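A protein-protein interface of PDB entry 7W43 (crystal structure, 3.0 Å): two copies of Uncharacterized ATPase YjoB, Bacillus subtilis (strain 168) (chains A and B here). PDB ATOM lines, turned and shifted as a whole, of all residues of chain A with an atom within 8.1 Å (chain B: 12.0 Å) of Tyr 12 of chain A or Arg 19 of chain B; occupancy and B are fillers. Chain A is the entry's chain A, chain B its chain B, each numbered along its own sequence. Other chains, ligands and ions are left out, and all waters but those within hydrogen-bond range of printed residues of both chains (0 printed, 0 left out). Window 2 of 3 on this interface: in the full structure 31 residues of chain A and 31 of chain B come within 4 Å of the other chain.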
ATOM      1  N   ILE A   9      12.455   6.926   8.506  1.00  0.00           N
ATOM      2  CA  ILE A   9      12.610   5.509   8.817  1.00  0.00           C
ATOM      3  C   ILE A   9      13.893   5.258   9.601  1.00  0.00           C
ATOM      4  O   ILE A   9      13.882   4.584  10.638  1.00  0.00           O
ATOM      5  CB  ILE A   9      12.565   4.676   7.521  1.00  0.00           C
ATOM      6  CG1 ILE A   9      11.174   4.742   6.888  1.00  0.00           C
ATOM      7  CG2 ILE A   9      12.981   3.237   7.790  1.00  0.00           C
ATOM      8  CD1 ILE A   9      10.043   4.405   7.843  1.00  0.00           C
ATOM      9  N   TYR A  10      15.015   5.792   9.124  1.00  0.00           N
ATOM     10  CA  TYR A  10      16.321   5.525   9.715  1.00  0.00           C
ATOM     11  C   TYR A  10      16.646   6.624  10.722  1.00  0.00           C
ATOM     12  O   TYR A  10      16.715   7.802  10.357  1.00  0.00           O
ATOM     13  CB  TYR A  10      17.382   5.436   8.616  1.00  0.00           C
ATOM     14  CG  TYR A  10      18.824   5.461   9.077  1.00  0.00           C
ATOM     15  CD1 TYR A  10      19.504   4.280   9.346  1.00  0.00           C
ATOM     16  CD2 TYR A  10      19.516   6.658   9.206  1.00  0.00           C
ATOM     17  CE1 TYR A  10      20.826   4.293   9.754  1.00  0.00           C
ATOM     18  CE2 TYR A  10      20.835   6.681   9.612  1.00  0.00           C
ATOM     19  CZ  TYR A  10      21.486   5.496   9.883  1.00  0.00           C
ATOM     20  OH  TYR A  10      22.801   5.515  10.287  1.00  0.00           O
ATOM     21  N   GLN A  11      16.842   6.239  11.984  1.00  0.00           N
ATOM     22  CA  GLN A  11      17.003   7.184  13.089  1.00  0.00           C
ATOM     23  C   GLN A  11      18.197   6.811  13.961  1.00  0.00           C
ATOM     24  O   GLN A  11      18.107   6.758  15.190  1.00  0.00           O
ATOM     25  CB  GLN A  11      15.747   7.249  13.957  1.00  0.00           C
ATOM     26  CG  GLN A  11      14.431   7.306  13.205  1.00  0.00           C
ATOM     27  CD  GLN A  11      13.238   7.127  14.125  1.00  0.00           C
ATOM     28  OE1 GLN A  11      12.090   7.185  13.687  1.00  0.00           O
ATOM     29  NE2 GLN A  11      13.506   6.913  15.409  1.00  0.00           N
ATOM     30  N   TYR A  12      19.344   6.551  13.343  1.00  0.00           N
ATOM     31  CA  TYR A  12      20.550   6.260  14.106  1.00  0.00           C
ATOM     32  C   TYR A  12      21.176   7.557  14.599  1.00  0.00           C
ATOM     33  O   TYR A  12      21.371   8.498  13.822  1.00  0.00           O
ATOM     34  CB  TYR A  12      21.552   5.478  13.257  1.00  0.00           C
ATOM     35  CG  TYR A  12      22.906   5.285  13.910  1.00  0.00           C
ATOM     36  CD1 TYR A  12      23.015   4.772  15.197  1.00  0.00           C
ATOM     37  CD2 TYR A  12      24.076   5.613  13.236  1.00  0.00           C
ATOM     38  CE1 TYR A  12      24.250   4.594  15.795  1.00  0.00           C
ATOM     39  CE2 TYR A  12      25.315   5.438  13.826  1.00  0.00           C
ATOM     40  CZ  TYR A  12      25.397   4.929  15.104  1.00  0.00           C
ATOM     41  OH  TYR A  12      26.628   4.753  15.694  1.00  0.00           O
ATOM     42  N   GLU A  13      21.481   7.610  15.892  1.00  0.00           N
ATOM     43  CA  GLU A  13      22.196   8.745  16.472  1.00  0.00           C
ATOM     44  C   GLU A  13      23.668   8.579  16.117  1.00  0.00           C
ATOM     45  O   GLU A  13      24.454   8.015  16.880  1.00  0.00           O
ATOM     46  CB  GLU A  13      21.985   8.809  17.980  1.00  0.00           C
ATOM     47  CG  GLU A  13      20.536   8.990  18.402  1.00  0.00           C
ATOM     48  CD  GLU A  13      20.388   9.162  19.902  1.00  0.00           C
ATOM     49  OE1 GLU A  13      19.244   9.318  20.374  1.00  0.00           O
ATOM     50  OE2 GLU A  13      21.419   9.149  20.608  1.00  0.00           O
ATOM     51  N   GLU A  14      24.039   9.063  14.932  1.00  0.00           N
ATOM     52  CA  GLU A  14      25.388   8.846  14.425  1.00  0.00           C
ATOM     53  C   GLU A  14      26.425   9.427  15.377  1.00  0.00           C
ATOM     54  O   GLU A  14      26.250  10.519  15.928  1.00  0.00           O
ATOM     55  CB  GLU A  14      25.538   9.454  13.026  1.00  0.00           C
ATOM     56  CG  GLU A  14      25.806  10.955  12.991  1.00  0.00           C
ATOM     57  CD  GLU A  14      26.053  11.466  11.589  1.00  0.00           C
ATOM     58  OE1 GLU A  14      25.496  10.876  10.640  1.00  0.00           O
ATOM     59  OE2 GLU A  14      26.804  12.451  11.432  1.00  0.00           O
ATOM     60  N   LYS A  15      27.495   8.671  15.601  1.00  0.00           N
ATOM     61  CA  LYS A  15      28.580   9.175  16.420  1.00  0.00           C
ATOM     62  C   LYS A  15      29.495  10.062  15.582  1.00  0.00           C
ATOM     63  O   LYS A  15      29.520   9.989  14.350  1.00  0.00           O
ATOM     64  CB  LYS A  15      29.365   8.025  17.056  1.00  0.00           C
ATOM     65  CG  LYS A  15      30.325   7.315  16.122  1.00  0.00           C
ATOM     66  CD  LYS A  15      30.605   5.899  16.601  1.00  0.00           C
ATOM     67  CE  LYS A  15      31.692   5.230  15.774  1.00  0.00           C
ATOM     68  NZ  LYS A  15      33.055   5.567  16.269  1.00  0.00           N
ATOM     69  N   GLU A  16      30.250  10.914  16.274  1.00  0.00           N
ATOM     70  CA  GLU A  16      31.020  11.953  15.599  1.00  0.00           C
ATOM     71  C   GLU A  16      32.111  11.372  14.709  1.00  0.00           C
ATOM     72  O   GLU A  16      32.477  11.986  13.700  1.00  0.00           O
ATOM     73  CB  GLU A  16      31.618  12.897  16.639  1.00  0.00           C
ATOM     74  CG  GLU A  16      30.672  13.175  17.795  1.00  0.00           C
ATOM     75  CD  GLU A  16      31.365  13.804  18.982  1.00  0.00           C
ATOM     76  OE1 GLU A  16      32.364  14.523  18.772  1.00  0.00           O
ATOM     77  OE2 GLU A  16      30.913  13.579  20.124  1.00  0.00           O
ATOM     78  N   GLU A  18      31.887   8.970  12.701  1.00  0.00           N
ATOM     79  CA  GLU A  18      31.320   8.614  11.405  1.00  0.00           C
ATOM     80  C   GLU A  18      31.276   9.789  10.437  1.00  0.00           C
ATOM     81  O   GLU A  18      30.993   9.580   9.253  1.00  0.00           O
ATOM     82  CB  GLU A  18      29.914   8.045  11.597  1.00  0.00           C
ATOM     83  CG  GLU A  18      29.831   7.014  12.708  1.00  0.00           C
ATOM     84  CD  GLU A  18      28.840   5.904  12.424  1.00  0.00           C
ATOM     85  OE1 GLU A  18      28.319   5.840  11.291  1.00  0.00           O
ATOM     86  OE2 GLU A  18      28.580   5.095  13.341  1.00  0.00           O
ATOM     87  N   TYR B  10      19.520 -17.615  11.109  1.00  0.00           N
ATOM     88  CA  TYR B  10      20.391 -16.563  11.618  1.00  0.00           C
ATOM     89  C   TYR B  10      19.842 -16.035  12.940  1.00  0.00           C
ATOM     90  O   TYR B  10      18.648 -15.742  13.050  1.00  0.00           O
ATOM     91  CB  TYR B  10      20.500 -15.443  10.583  1.00  0.00           C
ATOM     92  CG  TYR B  10      21.488 -14.342  10.897  1.00  0.00           C
ATOM     93  CD1 TYR B  10      21.080 -13.175  11.528  1.00  0.00           C
ATOM     94  CD2 TYR B  10      22.824 -14.457  10.533  1.00  0.00           C
ATOM     95  CE1 TYR B  10      21.975 -12.159  11.806  1.00  0.00           C
ATOM     96  CE2 TYR B  10      23.729 -13.444  10.807  1.00  0.00           C
ATOM     97  CZ  TYR B  10      23.297 -12.299  11.443  1.00  0.00           C
ATOM     98  OH  TYR B  10      24.187 -11.287  11.720  1.00  0.00           O
ATOM     99  N   TYR B  12      22.085 -13.807  15.131  1.00  0.00           N
ATOM    100  CA  TYR B  12      23.015 -12.869  15.738  1.00  0.00           C
ATOM    101  C   TYR B  12      22.297 -11.575  16.120  1.00  0.00           C
ATOM    102  O   TYR B  12      21.256 -11.216  15.565  1.00  0.00           O
ATOM    103  CB  TYR B  12      24.182 -12.568  14.798  1.00  0.00           C
ATOM    104  CG  TYR B  12      25.190 -11.599  15.375  1.00  0.00           C
ATOM    105  CD1 TYR B  12      25.847 -11.882  16.568  1.00  0.00           C
ATOM    106  CD2 TYR B  12      25.468 -10.395  14.746  1.00  0.00           C
ATOM    107  CE1 TYR B  12      26.764 -10.996  17.108  1.00  0.00           C
ATOM    108  CE2 TYR B  12      26.383  -9.504  15.279  1.00  0.00           C
ATOM    109  CZ  TYR B  12      27.027  -9.810  16.459  1.00  0.00           C
ATOM    110  OH  TYR B  12      27.937  -8.927  16.991  1.00  0.00           O
ATOM    111  N   GLU B  13      22.878 -10.871  17.085  1.00  0.00           N
ATOM    112  CA  GLU B  13      22.285  -9.681  17.677  1.00  0.00           C
ATOM    113  C   GLU B  13      22.854  -8.442  16.998  1.00  0.00           C
ATOM    114  O   GLU B  13      24.062  -8.192  17.072  1.00  0.00           O
ATOM    115  CB  GLU B  13      22.570  -9.651  19.177  1.00  0.00           C
ATOM    116  CG  GLU B  13      22.510 -11.022  19.831  1.00  0.00           C
ATOM    117  CD  GLU B  13      23.142 -11.039  21.206  1.00  0.00           C
ATOM    118  OE1 GLU B  13      24.360 -11.304  21.298  1.00  0.00           O
ATOM    119  OE2 GLU B  13      22.423 -10.790  22.195  1.00  0.00           O
ATOM    120  N   GLU B  14      21.991  -7.668  16.342  1.00  0.00           N
ATOM    121  CA  GLU B  14      22.446  -6.448  15.685  1.00  0.00           C
ATOM    122  C   GLU B  14      22.802  -5.399  16.733  1.00  0.00           C
ATOM    123  O   GLU B  14      21.976  -5.061  17.589  1.00  0.00           O
ATOM    124  CB  GLU B  14      21.378  -5.912  14.733  1.00  0.00           C
ATOM    125  CG  GLU B  14      19.948  -6.031  15.235  1.00  0.00           C
ATOM    126  CD  GLU B  14      18.937  -5.551  14.211  1.00  0.00           C
ATOM    127  OE1 GLU B  14      17.720  -5.651  14.479  1.00  0.00           O
ATOM    128  OE2 GLU B  14      19.358  -5.067  13.140  1.00  0.00           O
ATOM    129  N   LYS B  15      24.026  -4.889  16.669  1.00  0.00           N
ATOM    130  CA  LYS B  15      24.499  -3.882  17.606  1.00  0.00           C
ATOM    131  C   LYS B  15      24.183  -2.479  17.095  1.00  0.00           C
ATOM    132  O   LYS B  15      23.931  -2.265  15.907  1.00  0.00           O
ATOM    133  CB  LYS B  15      26.003  -4.032  17.842  1.00  0.00           C
ATOM    134  CG  LYS B  15      26.366  -4.853  19.073  1.00  0.00           C
ATOM    135  CD  LYS B  15      25.926  -6.304  18.938  1.00  0.00           C
ATOM    136  CE  LYS B  15      26.341  -7.122  20.152  1.00  0.00           C
ATOM    137  NZ  LYS B  15      26.008  -8.564  19.988  1.00  0.00           N
ATOM    138  N   GLU B  16      24.203  -1.512  18.018  1.00  0.00           N
ATOM    139  CA  GLU B  16      23.844  -0.145  17.653  1.00  0.00           C
ATOM    140  C   GLU B  16      24.916   0.504  16.787  1.00  0.00           C
ATOM    141  O   GLU B  16      24.600   1.326  15.921  1.00  0.00           O
ATOM    142  CB  GLU B  16      23.585   0.697  18.904  1.00  0.00           C
ATOM    143  CG  GLU B  16      23.809   2.192  18.694  1.00  0.00           C
ATOM    144  CD  GLU B  16      23.663   3.005  19.962  1.00  0.00           C
ATOM    145  OE1 GLU B  16      23.105   2.477  20.945  1.00  0.00           O
ATOM    146  OE2 GLU B  16      24.097   4.177  19.968  1.00  0.00           O
ATOM    147  N   ASN B  17      26.187   0.163  16.996  1.00  0.00           N
ATOM    148  CA  ASN B  17      27.200   0.669  16.079  1.00  0.00           C
ATOM    149  C   ASN B  17      27.145  -0.065  14.748  1.00  0.00           C
ATOM    150  O   ASN B  17      27.473   0.513  13.706  1.00  0.00           O
ATOM    151  CB  ASN B  17      28.592   0.565  16.700  1.00  0.00           C
ATOM    152  CG  ASN B  17      29.497   1.701  16.269  1.00  0.00           C
ATOM    153  OD1 ASN B  17      29.169   2.873  16.457  1.00  0.00           O
ATOM    154  ND2 ASN B  17      30.637   1.361  15.678  1.00  0.00           N
ATOM    155  N   GLU B  18      26.706  -1.322  14.759  1.00  0.00           N
ATOM    156  CA  GLU B  18      26.585  -2.111  13.543  1.00  0.00           C
ATOM    157  C   GLU B  18      25.316  -1.803  12.757  1.00  0.00           C
ATOM    158  O   GLU B  18      25.173  -2.295  11.633  1.00  0.00           O
ATOM    159  CB  GLU B  18      26.634  -3.602  13.885  1.00  0.00           C
ATOM    160  CG  GLU B  18      28.043  -4.163  14.024  1.00  0.00           C
ATOM    161  CD  GLU B  18      28.429  -5.077  12.875  1.00  0.00           C
ATOM    162  OE1 GLU B  18      27.561  -5.369  12.026  1.00  0.00           O
ATOM    163  OE2 GLU B  18      29.601  -5.506  12.819  1.00  0.00           O
ATOM    164  N   ARG B  19      24.393  -1.014  13.312  1.00  0.00           N
ATOM    165  CA  ARG B  19      23.188  -0.638  12.582  1.00  0.00           C
ATOM    166  C   ARG B  19      23.426   0.544  11.656  1.00  0.00           C
ATOM    167  O   ARG B  19      22.541   0.879  10.860  1.00  0.00           O
ATOM    168  CB  ARG B  19      22.064  -0.285  13.562  1.00  0.00           C
ATOM    169  CG  ARG B  19      22.246   1.085  14.184  1.00  0.00           C
ATOM    170  CD  ARG B  19      20.999   1.632  14.848  1.00  0.00           C
ATOM    171  NE  ARG B  19      20.301   0.606  15.610  1.00  0.00           N
ATOM    172  CZ  ARG B  19      19.027   0.682  15.975  1.00  0.00           C
ATOM    173  NH1 ARG B  19      18.304   1.748  15.664  1.00  0.00           N
ATOM    174  NH2 ARG B  19      18.480  -0.307  16.669  1.00  0.00           N
ATOM    175  N   ALA B  20      24.592   1.175  11.745  1.00  0.00           N
ATOM    176  CA  ALA B  20      24.862   2.393  10.997  1.00  0.00           C
ATOM    177  C   ALA B  20      24.937   2.118   9.501  1.00  0.00           C
ATOM    178  O   ALA B  20      25.409   1.067   9.058  1.00  0.00           O
ATOM    179  CB  ALA B  20      26.170   3.025  11.466  1.00  0.00           C
ATOM    180  N   ALA B  21      24.464   3.085   8.724  1.00  0.00           N
ATOM    181  CA  ALA B  21      24.643   3.062   7.282  1.00  0.00           C
ATOM    182  C   ALA B  21      26.064   3.478   6.919  1.00  0.00           C
ATOM    183  O   ALA B  21      26.720   4.236   7.641  1.00  0.00           O
ATOM    184  CB  ALA B  21      23.632   3.983   6.597  1.00  0.00           C
ATOM    185  N   ALA B  22      26.533   2.973   5.782  1.00  0.00           N
ATOM    186  CA  ALA B  22      27.914   3.148   5.346  1.00  0.00           C
ATOM    187  C   ALA B  22      28.017   4.372   4.446  1.00  0.00           C
ATOM    188  O   ALA B  22      27.447   4.392   3.349  1.00  0.00           O
ATOM    189  CB  ALA B  22      28.408   1.900   4.615  1.00  0.00           C
ATOM    190  N   GLY B  23      28.749   5.386   4.906  1.00  0.00           N
ATOM    191  CA  GLY B  23      28.969   6.586   4.129  1.00  0.00           C
ATOM    192  C   GLY B  23      27.901   7.648   4.260  1.00  0.00           C
ATOM    193  O   GLY B  23      28.083   8.752   3.730  1.00  0.00           O
ATOM    194  N   TYR B  24      26.791   7.358   4.942  1.00  0.00           N
ATOM    195  CA  TYR B  24      25.738   8.356   5.090  1.00  0.00           C
ATOM    196  C   TYR B  24      26.143   9.445   6.073  1.00  0.00           C
ATOM    197  O   TYR B  24      25.753  10.608   5.915  1.00  0.00           O
ATOM    198  CB  TYR B  24      24.439   7.694   5.545  1.00  0.00           C
ATOM    199  CG  TYR B  24      23.338   8.687   5.833  1.00  0.00           C
ATOM    200  CD1 TYR B  24      22.773   9.435   4.810  1.00  0.00           C
ATOM    201  CD2 TYR B  24      22.876   8.890   7.127  1.00  0.00           C
ATOM    202  CE1 TYR B  24      21.773  10.348   5.063  1.00  0.00           C
ATOM    203  CE2 TYR B  24      21.874   9.803   7.390  1.00  0.00           C
ATOM    204  CZ  TYR B  24      21.328  10.529   6.352  1.00  0.00           C
ATOM    205  OH  TYR B  24      20.331  11.441   6.596  1.00  0.00           O
ATOM    206  N   GLY B  25      26.922   9.084   7.098  1.00  0.00           N
ATOM    207  CA  GLY B  25      27.296  10.056   8.112  1.00  0.00           C
ATOM    208  C   GLY B  25      28.044  11.245   7.543  1.00  0.00           C
ATOM    209  O   GLY B  25      27.874  12.375   8.004  1.00  0.00           O
ATOM    210  N   THR B  26      28.880  11.010   6.529  1.00  0.00           N
ATOM    211  CA  THR B  26      29.594  12.106   5.886  1.00  0.00           C
ATOM    212  C   THR B  26      28.691  12.866   4.922  1.00  0.00           C
ATOM    213  O   THR B  26      28.729  14.102   4.877  1.00  0.00           O
ATOM    214  CB  THR B  26      30.826  11.581   5.150  1.00  0.00           C
ATOM    215  OG1 THR B  26      31.524  10.651   5.988  1.00  0.00           O
ATOM    216  CG2 THR B  26      31.759  12.727   4.792  1.00  0.00           C
ATOM    217  N   PHE B  27      27.881  12.149   4.140  1.00  0.00           N
ATOM    218  CA  PHE B  27      26.975  12.814   3.209  1.00  0.00           C
ATOM    219  C   PHE B  27      25.948  13.648   3.963  1.00  0.00           C
ATOM    220  O   PHE B  27      25.691  14.804   3.613  1.00  0.00           O
ATOM    221  CB  PHE B  27      26.287  11.783   2.311  1.00  0.00           C
ATOM    222  CG  PHE B  27      25.685  12.367   1.057  1.00  0.00           C
ATOM    223  CD1 PHE B  27      24.433  12.964   1.075  1.00  0.00           C
ATOM    224  CD2 PHE B  27      26.376  12.312  -0.143  1.00  0.00           C
ATOM    225  CE1 PHE B  27      23.886  13.493  -0.083  1.00  0.00           C
ATOM    226  CE2 PHE B  27      25.834  12.841  -1.300  1.00  0.00           C
ATOM    227  CZ  PHE B  27      24.588  13.432  -1.270  1.00  0.00           C
ATOM    228  N   GLY B  28      25.359  13.077   5.015  1.00  0.00           N
ATOM    229  CA  GLY B  28      24.410  13.834   5.819  1.00  0.00           C
ATOM    230  C   GLY B  28      25.045  15.034   6.494  1.00  0.00           C
ATOM    231  O   GLY B  28      24.519  16.147   6.427  1.00  0.00           O
ATOM    232  N   TYR B  29      26.188  14.819   7.155  1.00  0.00           N
ATOM    233  CA  TYR B  29      26.921  15.920   7.778  1.00  0.00           C
ATOM    234  C   TYR B  29      27.181  17.046   6.787  1.00  0.00           C
ATOM    235  O   TYR B  29      26.927  18.221   7.078  1.00  0.00           O
ATOM    236  CB  TYR B  29      28.245  15.413   8.355  1.00  0.00           C
ATOM    237  CG  TYR B  29      29.122  16.507   8.925  1.00  0.00           C
ATOM    238  CD1 TYR B  29      28.646  17.369   9.903  1.00  0.00           C
ATOM    239  CD2 TYR B  29      30.421  16.689   8.468  1.00  0.00           C
ATOM    240  CE1 TYR B  29      29.444  18.373  10.421  1.00  0.00           C
ATOM    241  CE2 TYR B  29      31.226  17.693   8.977  1.00  0.00           C
ATOM    242  CZ  TYR B  29      30.732  18.531   9.953  1.00  0.00           C
ATOM    243  OH  TYR B  29      31.526  19.532  10.466  1.00  0.00           O
ATOM    244  N   THR B  32      23.849  18.709   5.787  1.00  0.00           N
ATOM    245  CA  THR B  32      23.392  19.538   6.902  1.00  0.00           C
ATOM    246  C   THR B  32      24.202  20.825   6.993  1.00  0.00           C
ATOM    247  O   THR B  32      23.645  21.914   7.168  1.00  0.00           O
ATOM    248  CB  THR B  32      23.487  18.773   8.223  1.00  0.00           C
ATOM    249  OG1 THR B  32      24.808  18.244   8.383  1.00  0.00           O
ATOM    250  CG2 THR B  32      22.479  17.651   8.280  1.00  0.00           C
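The side-chain hydroxyl of Thr 26 of chain B is in hydrogen-bond range of the backbone carbonyl oxygen of Glu 18 of chain A. The side-chain amide oxygen (OD1) of Asn 17 of chain B sits at hydrogen-bond distance from the side-chain hydroxyl (OH) of Tyr 12 of chain A, at 3.3 Å. OH of Tyr 10 of chain A lies within hydrogen-bond range of N of Ala 21 of chain B, 3.3 Å away.
Of the 20 printed residues of chain B, 8 touch a printed residue of chain A. Printed residues of chain B that touch a printed residue of chain A: Glu 16, Asn 17, Arg 19, Ala 20, Ala 21, Tyr 24, Gly 25 and Thr 26. Hydrophobic or aromatic side chains of chain B within 4 Å of the printed part of chain A: Ala 20 and Tyr 24. Of the 9 printed residues of chain A, 5 touch a printed residue of chain B. Among the printed residues, 14 pairs touch across the chains.
Tyr 12 of chain A touches Glu 16 of chain B, but with the chains exchanged Glu 16 of chain A does not touch Tyr 12 of chain B (20.0 Å). Positions printed for both chains: 10, 12, 13, 14, 15, 16 and 18.
Of chain B, only Glu 16 (3.3 Å), Asn 17 (3.3 Å), Arg 19 (3.7 Å) and Ala 20 (3.5 Å) come within 4 Å of Tyr 12 of chain A. No residue of chain B comes within 4 Å of Gln 11 of chain A. No residue of chain B comes within 4 Å of Glu 13 of chain A. Of chain B, only Gly 25 comes within 4 Å of Glu 14 of chain A. Printed residues of chain B within 4 Å of Lys 15 of chain A: Asn 17. Ala 20 of chain B touches just these residues of chain A: Tyr 10 (3.8 Å), Tyr 12 (3.5 Å) and Glu 18 (3.5 Å). Of the printed residues of chain A, Asn 17 of chain B touches Tyr 12, Lys 15 and Glu 18. Printed residues of chain B within 4 Å of Glu 18 of chain A: Asn 17, Ala 20, Gly 25 and Thr 26. Of the printed residues of chain A, Tyr 24 of chain B touches Tyr 10 (3.9 Å). Thr 32 of chain B touches none of the printed residues of chain A. Glu 16 of chain A touches none of the printed residues of chain B. The nearest residue of chain B that does not touch Tyr 12 of chain A is Ala 21 of chain B (5.2 Å).
CE1 of Tyr 10 of chain A touches O of Arg 19 of chain B, 3.98 Å away. OH of Tyr 10 of chain A touches CA of Ala 20 of chain B, 3.8 Å away. Tyr 10 of chain A touches Tyr 24 of chain B. Tyr 12 of chain A touches Glu 16 of chain B (CE1 to O, 3.3 Å). CD1 of Tyr 12 of chain A touches CD of Arg 19 of chain B (3.7 Å). Ala 20 of chain B touches Tyr 12 of chain A. Glu 14 of chain A touches Gly 25 of chain B (OE1 to CA, 3.2 Å). Lys 15 of chain A touches Asn 17 of chain B. Glu 18 of chain A touches Ala 20 of chain B. Gly 25 of chain B touches Glu 18 of chain A (C to O, 3.8 Å).
The side-chain carboxylate (OE2) of Glu 18 of chain A is in hydrogen-bond range of the side-chain hydroxyl (OH) of Tyr 12 of chain A (3.1 Å).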
